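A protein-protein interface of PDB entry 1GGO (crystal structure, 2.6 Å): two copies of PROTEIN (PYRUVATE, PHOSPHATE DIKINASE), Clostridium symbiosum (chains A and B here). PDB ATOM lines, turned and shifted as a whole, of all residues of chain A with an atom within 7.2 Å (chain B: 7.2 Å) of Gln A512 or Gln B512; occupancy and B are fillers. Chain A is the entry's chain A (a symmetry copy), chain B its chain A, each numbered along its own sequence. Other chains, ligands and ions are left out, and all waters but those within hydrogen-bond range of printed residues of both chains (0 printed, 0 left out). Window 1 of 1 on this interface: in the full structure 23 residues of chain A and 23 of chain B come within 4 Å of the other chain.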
ATOM      1  N   LEU A 376     -12.640  25.105  28.129  1.00  0.00           N
ATOM      2  CA  LEU A 376     -11.233  25.173  27.750  1.00  0.00           C
ATOM      3  C   LEU A 376     -10.160  24.985  28.804  1.00  0.00           C
ATOM      4  O   LEU A 376      -8.978  25.065  28.472  1.00  0.00           O
ATOM      5  CB  LEU A 376     -10.982  26.478  26.983  1.00  0.00           C
ATOM      6  CG  LEU A 376     -11.806  26.412  25.680  1.00  0.00           C
ATOM      7  CD1 LEU A 376     -12.023  27.785  25.098  1.00  0.00           C
ATOM      8  CD2 LEU A 376     -11.110  25.511  24.669  1.00  0.00           C
ATOM      9  N   HIS A 377     -10.552  24.731  30.055  1.00  0.00           N
ATOM     10  CA  HIS A 377      -9.568  24.508  31.115  1.00  0.00           C
ATOM     11  C   HIS A 377      -8.789  23.258  30.709  1.00  0.00           C
ATOM     12  O   HIS A 377      -9.379  22.243  30.334  1.00  0.00           O
ATOM     13  CB  HIS A 377     -10.244  24.272  32.468  1.00  0.00           C
ATOM     14  CG  HIS A 377     -10.984  25.458  32.999  1.00  0.00           C
ATOM     15  ND1 HIS A 377     -11.576  25.471  34.251  1.00  0.00           N
ATOM     16  CD2 HIS A 377     -11.268  26.664  32.448  1.00  0.00           C
ATOM     17  CE1 HIS A 377     -12.191  26.631  34.436  1.00  0.00           C
ATOM     18  NE2 HIS A 377     -12.018  27.365  33.359  1.00  0.00           N
ATOM     19  N   PRO A 378      -7.449  23.310  30.779  1.00  0.00           N
ATOM     20  CA  PRO A 378      -6.600  22.174  30.408  1.00  0.00           C
ATOM     21  C   PRO A 378      -6.831  20.882  31.187  1.00  0.00           C
ATOM     22  O   PRO A 378      -6.573  20.821  32.382  1.00  0.00           O
ATOM     23  CB  PRO A 378      -5.189  22.719  30.613  1.00  0.00           C
ATOM     24  CG  PRO A 378      -5.380  23.665  31.761  1.00  0.00           C
ATOM     25  CD  PRO A 378      -6.636  24.394  31.351  1.00  0.00           C
ATOM     26  N   THR A 379      -7.318  19.851  30.515  1.00  0.00           N
ATOM     27  CA  THR A 379      -7.529  18.572  31.173  1.00  0.00           C
ATOM     28  C   THR A 379      -6.149  18.007  31.535  1.00  0.00           C
ATOM     29  O   THR A 379      -5.121  18.596  31.187  1.00  0.00           O
ATOM     30  CB  THR A 379      -8.287  17.605  30.232  1.00  0.00           C
ATOM     31  OG1 THR A 379      -7.628  17.558  28.957  1.00  0.00           O
ATOM     32  CG2 THR A 379      -9.736  18.091  30.023  1.00  0.00           C
ATOM     33  N   PHE A 380      -6.110  16.889  32.252  1.00  0.00           N
ATOM     34  CA  PHE A 380      -4.831  16.289  32.632  1.00  0.00           C
ATOM     35  C   PHE A 380      -4.280  15.591  31.408  1.00  0.00           C
ATOM     36  O   PHE A 380      -4.987  15.443  30.409  1.00  0.00           O
ATOM     37  CB  PHE A 380      -5.000  15.236  33.737  1.00  0.00           C
ATOM     38  CG  PHE A 380      -4.992  15.792  35.126  1.00  0.00           C
ATOM     39  CD1 PHE A 380      -4.118  16.808  35.481  1.00  0.00           C
ATOM     40  CD2 PHE A 380      -5.845  15.275  36.103  1.00  0.00           C
ATOM     41  CE1 PHE A 380      -4.090  17.306  36.783  1.00  0.00           C
ATOM     42  CE2 PHE A 380      -5.823  15.770  37.411  1.00  0.00           C
ATOM     43  CZ  PHE A 380      -4.945  16.784  37.744  1.00  0.00           C
ATOM     44  N   ASN A 381      -3.024  15.162  31.497  1.00  0.00           N
ATOM     45  CA  ASN A 381      -2.383  14.436  30.404  1.00  0.00           C
ATOM     46  C   ASN A 381      -2.446  12.968  30.793  1.00  0.00           C
ATOM     47  O   ASN A 381      -1.885  12.561  31.807  1.00  0.00           O
ATOM     48  CB  ASN A 381      -0.920  14.860  30.236  1.00  0.00           C
ATOM     49  CG  ASN A 381      -0.262  14.218  29.016  1.00  0.00           C
ATOM     50  OD1 ASN A 381      -0.720  14.388  27.882  1.00  0.00           O
ATOM     51  ND2 ASN A 381       0.833  13.488  29.245  1.00  0.00           N
ATOM     52  N   PRO A 382      -3.137  12.154  29.988  1.00  0.00           N
ATOM     53  CA  PRO A 382      -3.281  10.726  30.250  1.00  0.00           C
ATOM     54  C   PRO A 382      -2.020  10.049  30.800  1.00  0.00           C
ATOM     55  O   PRO A 382      -2.050   9.467  31.887  1.00  0.00           O
ATOM     56  CB  PRO A 382      -3.704  10.177  28.890  1.00  0.00           C
ATOM     57  CG  PRO A 382      -3.119  11.147  27.938  1.00  0.00           C
ATOM     58  CD  PRO A 382      -3.455  12.441  28.583  1.00  0.00           C
ATOM     59  N   ALA A 383      -0.920  10.125  30.054  1.00  0.00           N
ATOM     60  CA  ALA A 383       0.326   9.503  30.482  1.00  0.00           C
ATOM     61  C   ALA A 383       0.724   9.991  31.860  1.00  0.00           C
ATOM     62  O   ALA A 383       1.269   9.230  32.653  1.00  0.00           O
ATOM     63  CB  ALA A 383       1.425   9.800  29.494  1.00  0.00           C
ATOM     64  N   ILE A 509       0.368  17.165  38.561  1.00  0.00           N
ATOM     65  CA  ILE A 509       0.239  16.342  37.310  1.00  0.00           C
ATOM     66  C   ILE A 509       0.088  17.193  36.030  1.00  0.00           C
ATOM     67  O   ILE A 509      -0.732  18.126  35.972  1.00  0.00           O
ATOM     68  CB  ILE A 509      -0.936  15.342  37.365  1.00  0.00           C
ATOM     69  CG1 ILE A 509      -0.602  14.236  38.384  1.00  0.00           C
ATOM     70  CG2 ILE A 509      -1.196  14.753  35.957  1.00  0.00           C
ATOM     71  CD1 ILE A 509      -1.501  13.011  38.295  1.00  0.00           C
ATOM     72  N   GLU A 510       0.831  16.818  34.984  1.00  0.00           N
ATOM     73  CA  GLU A 510       0.769  17.523  33.712  1.00  0.00           C
ATOM     74  C   GLU A 510      -0.633  17.634  33.118  1.00  0.00           C
ATOM     75  O   GLU A 510      -1.310  16.635  32.906  1.00  0.00           O
ATOM     76  CB  GLU A 510       1.703  16.873  32.694  1.00  0.00           C
ATOM     77  CG  GLU A 510       1.892  17.697  31.431  1.00  0.00           C
ATOM     78  CD  GLU A 510       2.553  16.914  30.329  1.00  0.00           C
ATOM     79  OE1 GLU A 510       3.701  16.445  30.530  1.00  0.00           O
ATOM     80  OE2 GLU A 510       1.919  16.753  29.256  1.00  0.00           O
ATOM     81  N   THR A 511      -1.045  18.869  32.868  1.00  0.00           N
ATOM     82  CA  THR A 511      -2.341  19.173  32.264  1.00  0.00           C
ATOM     83  C   THR A 511      -1.979  19.529  30.834  1.00  0.00           C
ATOM     84  O   THR A 511      -0.826  19.829  30.566  1.00  0.00           O
ATOM     85  CB  THR A 511      -2.988  20.379  32.958  1.00  0.00           C
ATOM     86  OG1 THR A 511      -1.977  21.078  33.696  1.00  0.00           O
ATOM     87  CG2 THR A 511      -4.085  19.921  33.909  1.00  0.00           C
ATOM     88  N   GLN A 512      -2.922  19.510  29.902  1.00  0.00           N
ATOM     89  CA  GLN A 512      -2.520  19.857  28.549  1.00  0.00           C
ATOM     90  C   GLN A 512      -3.375  20.875  27.818  1.00  0.00           C
ATOM     91  O   GLN A 512      -3.024  22.055  27.775  1.00  0.00           O
ATOM     92  CB  GLN A 512      -2.353  18.593  27.694  1.00  0.00           C
ATOM     93  CG  GLN A 512      -3.583  17.739  27.515  1.00  0.00           C
ATOM     94  CD  GLN A 512      -3.307  16.507  26.670  1.00  0.00           C
ATOM     95  OE1 GLN A 512      -4.216  15.747  26.345  1.00  0.00           O
ATOM     96  NE2 GLN A 512      -2.039  16.304  26.308  1.00  0.00           N
ATOM     97  N   GLU A 513      -4.484  20.430  27.239  1.00  0.00           N
ATOM     98  CA  GLU A 513      -5.384  21.311  26.492  1.00  0.00           C
ATOM     99  C   GLU A 513      -6.252  20.282  25.798  1.00  0.00           C
ATOM    100  O   GLU A 513      -5.813  19.140  25.661  1.00  0.00           O
ATOM    101  CB  GLU A 513      -4.594  22.140  25.459  1.00  0.00           C
ATOM    102  CG  GLU A 513      -5.191  23.515  25.094  1.00  0.00           C
ATOM    103  CD  GLU A 513      -4.273  24.356  24.178  1.00  0.00           C
ATOM    104  OE1 GLU A 513      -3.185  24.801  24.616  1.00  0.00           O
ATOM    105  OE2 GLU A 513      -4.638  24.589  23.008  1.00  0.00           O
ATOM    106  N   ALA A 514      -7.457  20.629  25.359  1.00  0.00           N
ATOM    107  CA  ALA A 514      -8.240  19.584  24.715  1.00  0.00           C
ATOM    108  C   ALA A 514      -9.571  19.918  24.079  1.00  0.00           C
ATOM    109  O   ALA A 514     -10.164  20.967  24.308  1.00  0.00           O
ATOM    110  CB  ALA A 514      -8.439  18.420  25.684  1.00  0.00           C
ATOM    111  N   LEU B 376     -10.696   7.775  15.236  1.00  0.00           N
ATOM    112  CA  LEU B 376     -10.093   7.294  16.474  1.00  0.00           C
ATOM    113  C   LEU B 376      -8.616   6.956  16.510  1.00  0.00           C
ATOM    114  O   LEU B 376      -8.126   6.532  17.556  1.00  0.00           O
ATOM    115  CB  LEU B 376     -10.908   6.104  17.000  1.00  0.00           C
ATOM    116  CG  LEU B 376     -12.317   6.629  17.349  1.00  0.00           C
ATOM    117  CD1 LEU B 376     -13.320   5.508  17.409  1.00  0.00           C
ATOM    118  CD2 LEU B 376     -12.279   7.380  18.673  1.00  0.00           C
ATOM    119  N   HIS B 377      -7.905   7.145  15.395  1.00  0.00           N
ATOM    120  CA  HIS B 377      -6.468   6.870  15.370  1.00  0.00           C
ATOM    121  C   HIS B 377      -5.838   7.830  16.378  1.00  0.00           C
ATOM    122  O   HIS B 377      -6.133   9.027  16.375  1.00  0.00           O
ATOM    123  CB  HIS B 377      -5.872   7.123  13.983  1.00  0.00           C
ATOM    124  CG  HIS B 377      -6.368   6.190  12.923  1.00  0.00           C
ATOM    125  ND1 HIS B 377      -5.874   6.198  11.630  1.00  0.00           N
ATOM    126  CD2 HIS B 377      -7.338   5.243  12.939  1.00  0.00           C
ATOM    127  CE1 HIS B 377      -6.524   5.298  10.904  1.00  0.00           C
ATOM    128  NE2 HIS B 377      -7.412   4.711  11.675  1.00  0.00           N
ATOM    129  N   PRO B 378      -4.959   7.321  17.256  1.00  0.00           N
ATOM    130  CA  PRO B 378      -4.299   8.147  18.272  1.00  0.00           C
ATOM    131  C   PRO B 378      -3.468   9.315  17.749  1.00  0.00           C
ATOM    132  O   PRO B 378      -2.451   9.114  17.100  1.00  0.00           O
ATOM    133  CB  PRO B 378      -3.447   7.136  19.034  1.00  0.00           C
ATOM    134  CG  PRO B 378      -3.085   6.155  17.959  1.00  0.00           C
ATOM    135  CD  PRO B 378      -4.410   5.957  17.266  1.00  0.00           C
ATOM    136  N   THR B 379      -3.899  10.535  18.030  1.00  0.00           N
ATOM    137  CA  THR B 379      -3.144  11.702  17.604  1.00  0.00           C
ATOM    138  C   THR B 379      -1.828  11.712  18.394  1.00  0.00           C
ATOM    139  O   THR B 379      -1.618  10.869  19.271  1.00  0.00           O
ATOM    140  CB  THR B 379      -3.955  12.992  17.874  1.00  0.00           C
ATOM    141  OG1 THR B 379      -4.411  12.997  19.235  1.00  0.00           O
ATOM    142  CG2 THR B 379      -5.181  13.056  16.940  1.00  0.00           C
ATOM    143  N   PHE B 380      -0.927  12.637  18.078  1.00  0.00           N
ATOM    144  CA  PHE B 380       0.349  12.711  18.790  1.00  0.00           C
ATOM    145  C   PHE B 380       0.078  13.352  20.134  1.00  0.00           C
ATOM    146  O   PHE B 380      -1.017  13.870  20.363  1.00  0.00           O
ATOM    147  CB  PHE B 380       1.367  13.590  18.048  1.00  0.00           C
ATOM    148  CG  PHE B 380       2.154  12.871  16.999  1.00  0.00           C
ATOM    149  CD1 PHE B 380       2.613  11.580  17.215  1.00  0.00           C
ATOM    150  CD2 PHE B 380       2.469  13.498  15.792  1.00  0.00           C
ATOM    151  CE1 PHE B 380       3.372  10.920  16.248  1.00  0.00           C
ATOM    152  CE2 PHE B 380       3.230  12.841  14.819  1.00  0.00           C
ATOM    153  CZ  PHE B 380       3.677  11.555  15.052  1.00  0.00           C
ATOM    154  N   ASN B 381       1.078  13.317  21.010  1.00  0.00           N
ATOM    155  CA  ASN B 381       0.965  13.934  22.329  1.00  0.00           C
ATOM    156  C   ASN B 381       1.690  15.266  22.222  1.00  0.00           C
ATOM    157  O   ASN B 381       2.889  15.310  21.960  1.00  0.00           O
ATOM    158  CB  ASN B 381       1.631  13.072  23.406  1.00  0.00           C
ATOM    159  CG  ASN B 381       1.412  13.623  24.814  1.00  0.00           C
ATOM    160  OD1 ASN B 381       0.273  13.782  25.265  1.00  0.00           O
ATOM    161  ND2 ASN B 381       2.509  13.903  25.522  1.00  0.00           N
ATOM    162  N   PRO B 382       0.964  16.372  22.422  1.00  0.00           N
ATOM    163  CA  PRO B 382       1.536  17.711  22.342  1.00  0.00           C
ATOM    164  C   PRO B 382       2.944  17.839  22.933  1.00  0.00           C
ATOM    165  O   PRO B 382       3.880  18.235  22.233  1.00  0.00           O
ATOM    166  CB  PRO B 382       0.504  18.559  23.081  1.00  0.00           C
ATOM    167  CG  PRO B 382      -0.116  17.597  24.017  1.00  0.00           C
ATOM    168  CD  PRO B 382      -0.314  16.412  23.145  1.00  0.00           C
ATOM    169  N   ALA B 383       3.095  17.505  24.214  1.00  0.00           N
ATOM    170  CA  ALA B 383       4.391  17.605  24.872  1.00  0.00           C
ATOM    171  C   ALA B 383       5.440  16.819  24.113  1.00  0.00           C
ATOM    172  O   ALA B 383       6.594  17.230  24.046  1.00  0.00           O
ATOM    173  CB  ALA B 383       4.297  17.100  26.289  1.00  0.00           C
ATOM    174  N   ILE B 509       7.481   9.298  18.131  1.00  0.00           N
ATOM    175  CA  ILE B 509       6.802  10.287  19.037  1.00  0.00           C
ATOM    176  C   ILE B 509       5.528   9.730  19.708  1.00  0.00           C
ATOM    177  O   ILE B 509       4.656   9.145  19.043  1.00  0.00           O
ATOM    178  CB  ILE B 509       6.433  11.605  18.323  1.00  0.00           C
ATOM    179  CG1 ILE B 509       7.728  12.376  18.000  1.00  0.00           C
ATOM    180  CG2 ILE B 509       5.484  12.443  19.214  1.00  0.00           C
ATOM    181  CD1 ILE B 509       7.508  13.831  17.611  1.00  0.00           C
ATOM    182  N   GLU B 510       5.394   9.980  21.015  1.00  0.00           N
ATOM    183  CA  GLU B 510       4.230   9.527  21.763  1.00  0.00           C
ATOM    184  C   GLU B 510       2.892   9.980  21.185  1.00  0.00           C
ATOM    185  O   GLU B 510       2.651  11.167  21.005  1.00  0.00           O
ATOM    186  CB  GLU B 510       4.329   9.964  23.222  1.00  0.00           C
ATOM    187  CG  GLU B 510       3.291   9.314  24.123  1.00  0.00           C
ATOM    188  CD  GLU B 510       3.203   9.980  25.469  1.00  0.00           C
ATOM    189  OE1 GLU B 510       4.227  10.002  26.197  1.00  0.00           O
ATOM    190  OE2 GLU B 510       2.108  10.497  25.803  1.00  0.00           O
ATOM    191  N   THR B 511       2.042   9.004  20.896  1.00  0.00           N
ATOM    192  CA  THR B 511       0.698   9.243  20.372  1.00  0.00           C
ATOM    193  C   THR B 511      -0.190   8.995  21.577  1.00  0.00           C
ATOM    194  O   THR B 511       0.252   8.367  22.527  1.00  0.00           O
ATOM    195  CB  THR B 511       0.368   8.238  19.260  1.00  0.00           C
ATOM    196  OG1 THR B 511       1.287   7.142  19.348  1.00  0.00           O
ATOM    197  CG2 THR B 511       0.491   8.896  17.894  1.00  0.00           C
ATOM    198  N   GLN B 512      -1.431   9.464  21.576  1.00  0.00           N
ATOM    199  CA  GLN B 512      -2.237   9.200  22.756  1.00  0.00           C
ATOM    200  C   GLN B 512      -3.630   8.644  22.526  1.00  0.00           C
ATOM    201  O   GLN B 512      -3.834   7.435  22.631  1.00  0.00           O
ATOM    202  CB  GLN B 512      -2.303  10.443  23.654  1.00  0.00           C
ATOM    203  CG  GLN B 512      -2.919  11.677  23.044  1.00  0.00           C
ATOM    204  CD  GLN B 512      -2.921  12.852  24.007  1.00  0.00           C
ATOM    205  OE1 GLN B 512      -3.467  13.911  23.710  1.00  0.00           O
ATOM    206  NE2 GLN B 512      -2.302  12.668  25.174  1.00  0.00           N
ATOM    207  N   GLU B 513      -4.586   9.514  22.222  1.00  0.00           N
ATOM    208  CA  GLU B 513      -5.973   9.104  21.992  1.00  0.00           C
ATOM    209  C   GLU B 513      -6.661  10.453  22.022  1.00  0.00           C
ATOM    210  O   GLU B 513      -6.095  11.389  22.588  1.00  0.00           O
ATOM    211  CB  GLU B 513      -6.472   8.215  23.150  1.00  0.00           C
ATOM    212  CG  GLU B 513      -7.567   7.188  22.791  1.00  0.00           C
ATOM    213  CD  GLU B 513      -7.908   6.228  23.955  1.00  0.00           C
ATOM    214  OE1 GLU B 513      -7.063   5.386  24.342  1.00  0.00           O
ATOM    215  OE2 GLU B 513      -9.033   6.303  24.487  1.00  0.00           O
ATOM    216  N   ALA B 514      -7.846  10.598  21.439  1.00  0.00           N
ATOM    217  CA  ALA B 514      -8.440  11.926  21.495  1.00  0.00           C
ATOM    218  C   ALA B 514      -9.837  12.154  20.964  1.00  0.00           C
ATOM    219  O   ALA B 514     -10.406  11.343  20.239  1.00  0.00           O
ATOM    220  CB  ALA B 514      -7.498  12.938  20.843  1.00  0.00           C
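The side-chain amide oxygen (OD1) of Asn B381 sits close to the side-chain amide oxygen (OD1) of Asn A381 (2.9 Å). The side-chain amide oxygen (OE1) of Gln B512 lies close to the side-chain amide oxygen (OE1) of Gln A512, 3.3 Å away.
O of Thr B379 sits at hydrogen-bond distance from N of Gln B512 (2.7 Å). The backbone NH (N) of Asn B381 sits at hydrogen-bond distance from the backbone carbonyl oxygen (O) of Glu B510 (2.7 Å). The side-chain amide oxygen (OD1) of Asn B381 is in hydrogen-bond range of the side-chain amide nitrogen (NE2) of Gln B512. The backbone carbonyl oxygen (O) of Thr A379 sits at hydrogen-bond distance from the backbone NH (N) of Gln A512 (2.7 Å). The backbone NH (N) of Asn A381 lies within hydrogen-bond range of the backbone carbonyl oxygen (O) of Glu A510 (2.7 Å). OD1 of Asn A381 sits at hydrogen-bond distance from NE2 of Gln A512 (2.8 Å).
OD1 of Asn A381 touches NE2 of Gln B512, 3.6 Å away. Gln B512 touches Pro A382 (NE2 to CG, 3.3 Å). Ala A383 touches Glu B510 (CB to OE2, 3.8 Å). Ala B383 touches Glu A510. Gln A512 touches Asn B381. Pro B382 touches Gln A512 (CG to NE2, 3.3 Å).
Printed residues of chain B within 4 Å of Asn A381: Asn B381 and Gln B512. Of chain B, only Asn B381 (3.6 Å), Pro B382 (3.3 Å) and Gln B512 (3.3 Å) come within 4 Å of Gln A512. Printed residues of chain A within 4 Å of Asn B381: Asn A381 (2.9 Å) and Gln A512 (3.6 Å). Of the printed residues of chain A, Pro B382 touches Gln A512. Of the printed residues of chain A, Ala B383 touches Glu A510 (3.8 Å). Of the printed residues of chain A, Glu B510 touches Ala A383 (3.8 Å). Gln B512 touches just these residues of chain A: Asn A381 (3.6 Å), Pro A382 (3.3 Å) and Gln A512 (3.3 Å). The nearest residue of chain B that does not touch Gln A512 is Ala B383 (5.7 Å). The nearest printed residue of chain B that does not touch Pro A382 is Asn B381 (5.1 Å).
Hydrophobic or aromatic side chains of chain B within 4 Å of the printed part of chain A: Pro B382 and Ala B383. Along chain B the printed residues that touch a printed residue of chain A span positions 381 to 512. Hydrophobic or aromatic side chains of chain A within 4 Å of the printed part of chain B: Pro A382 and Ala A383.
Asn A381 touches Gln B512, and with the chains exchanged Gln A512 touches Asn B381. Pro A382 touches Gln B512, and with the chains exchanged Gln A512 touches Pro B382. Ala A383 touches Glu B510, and with the chains exchanged Glu A510 touches Ala B383. Gln B512 touches its own counterpart, Gln A512. Of the 8 pairs that touch across the chains among the printed residues, 8 have their exchanged pair printed and touching as well.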
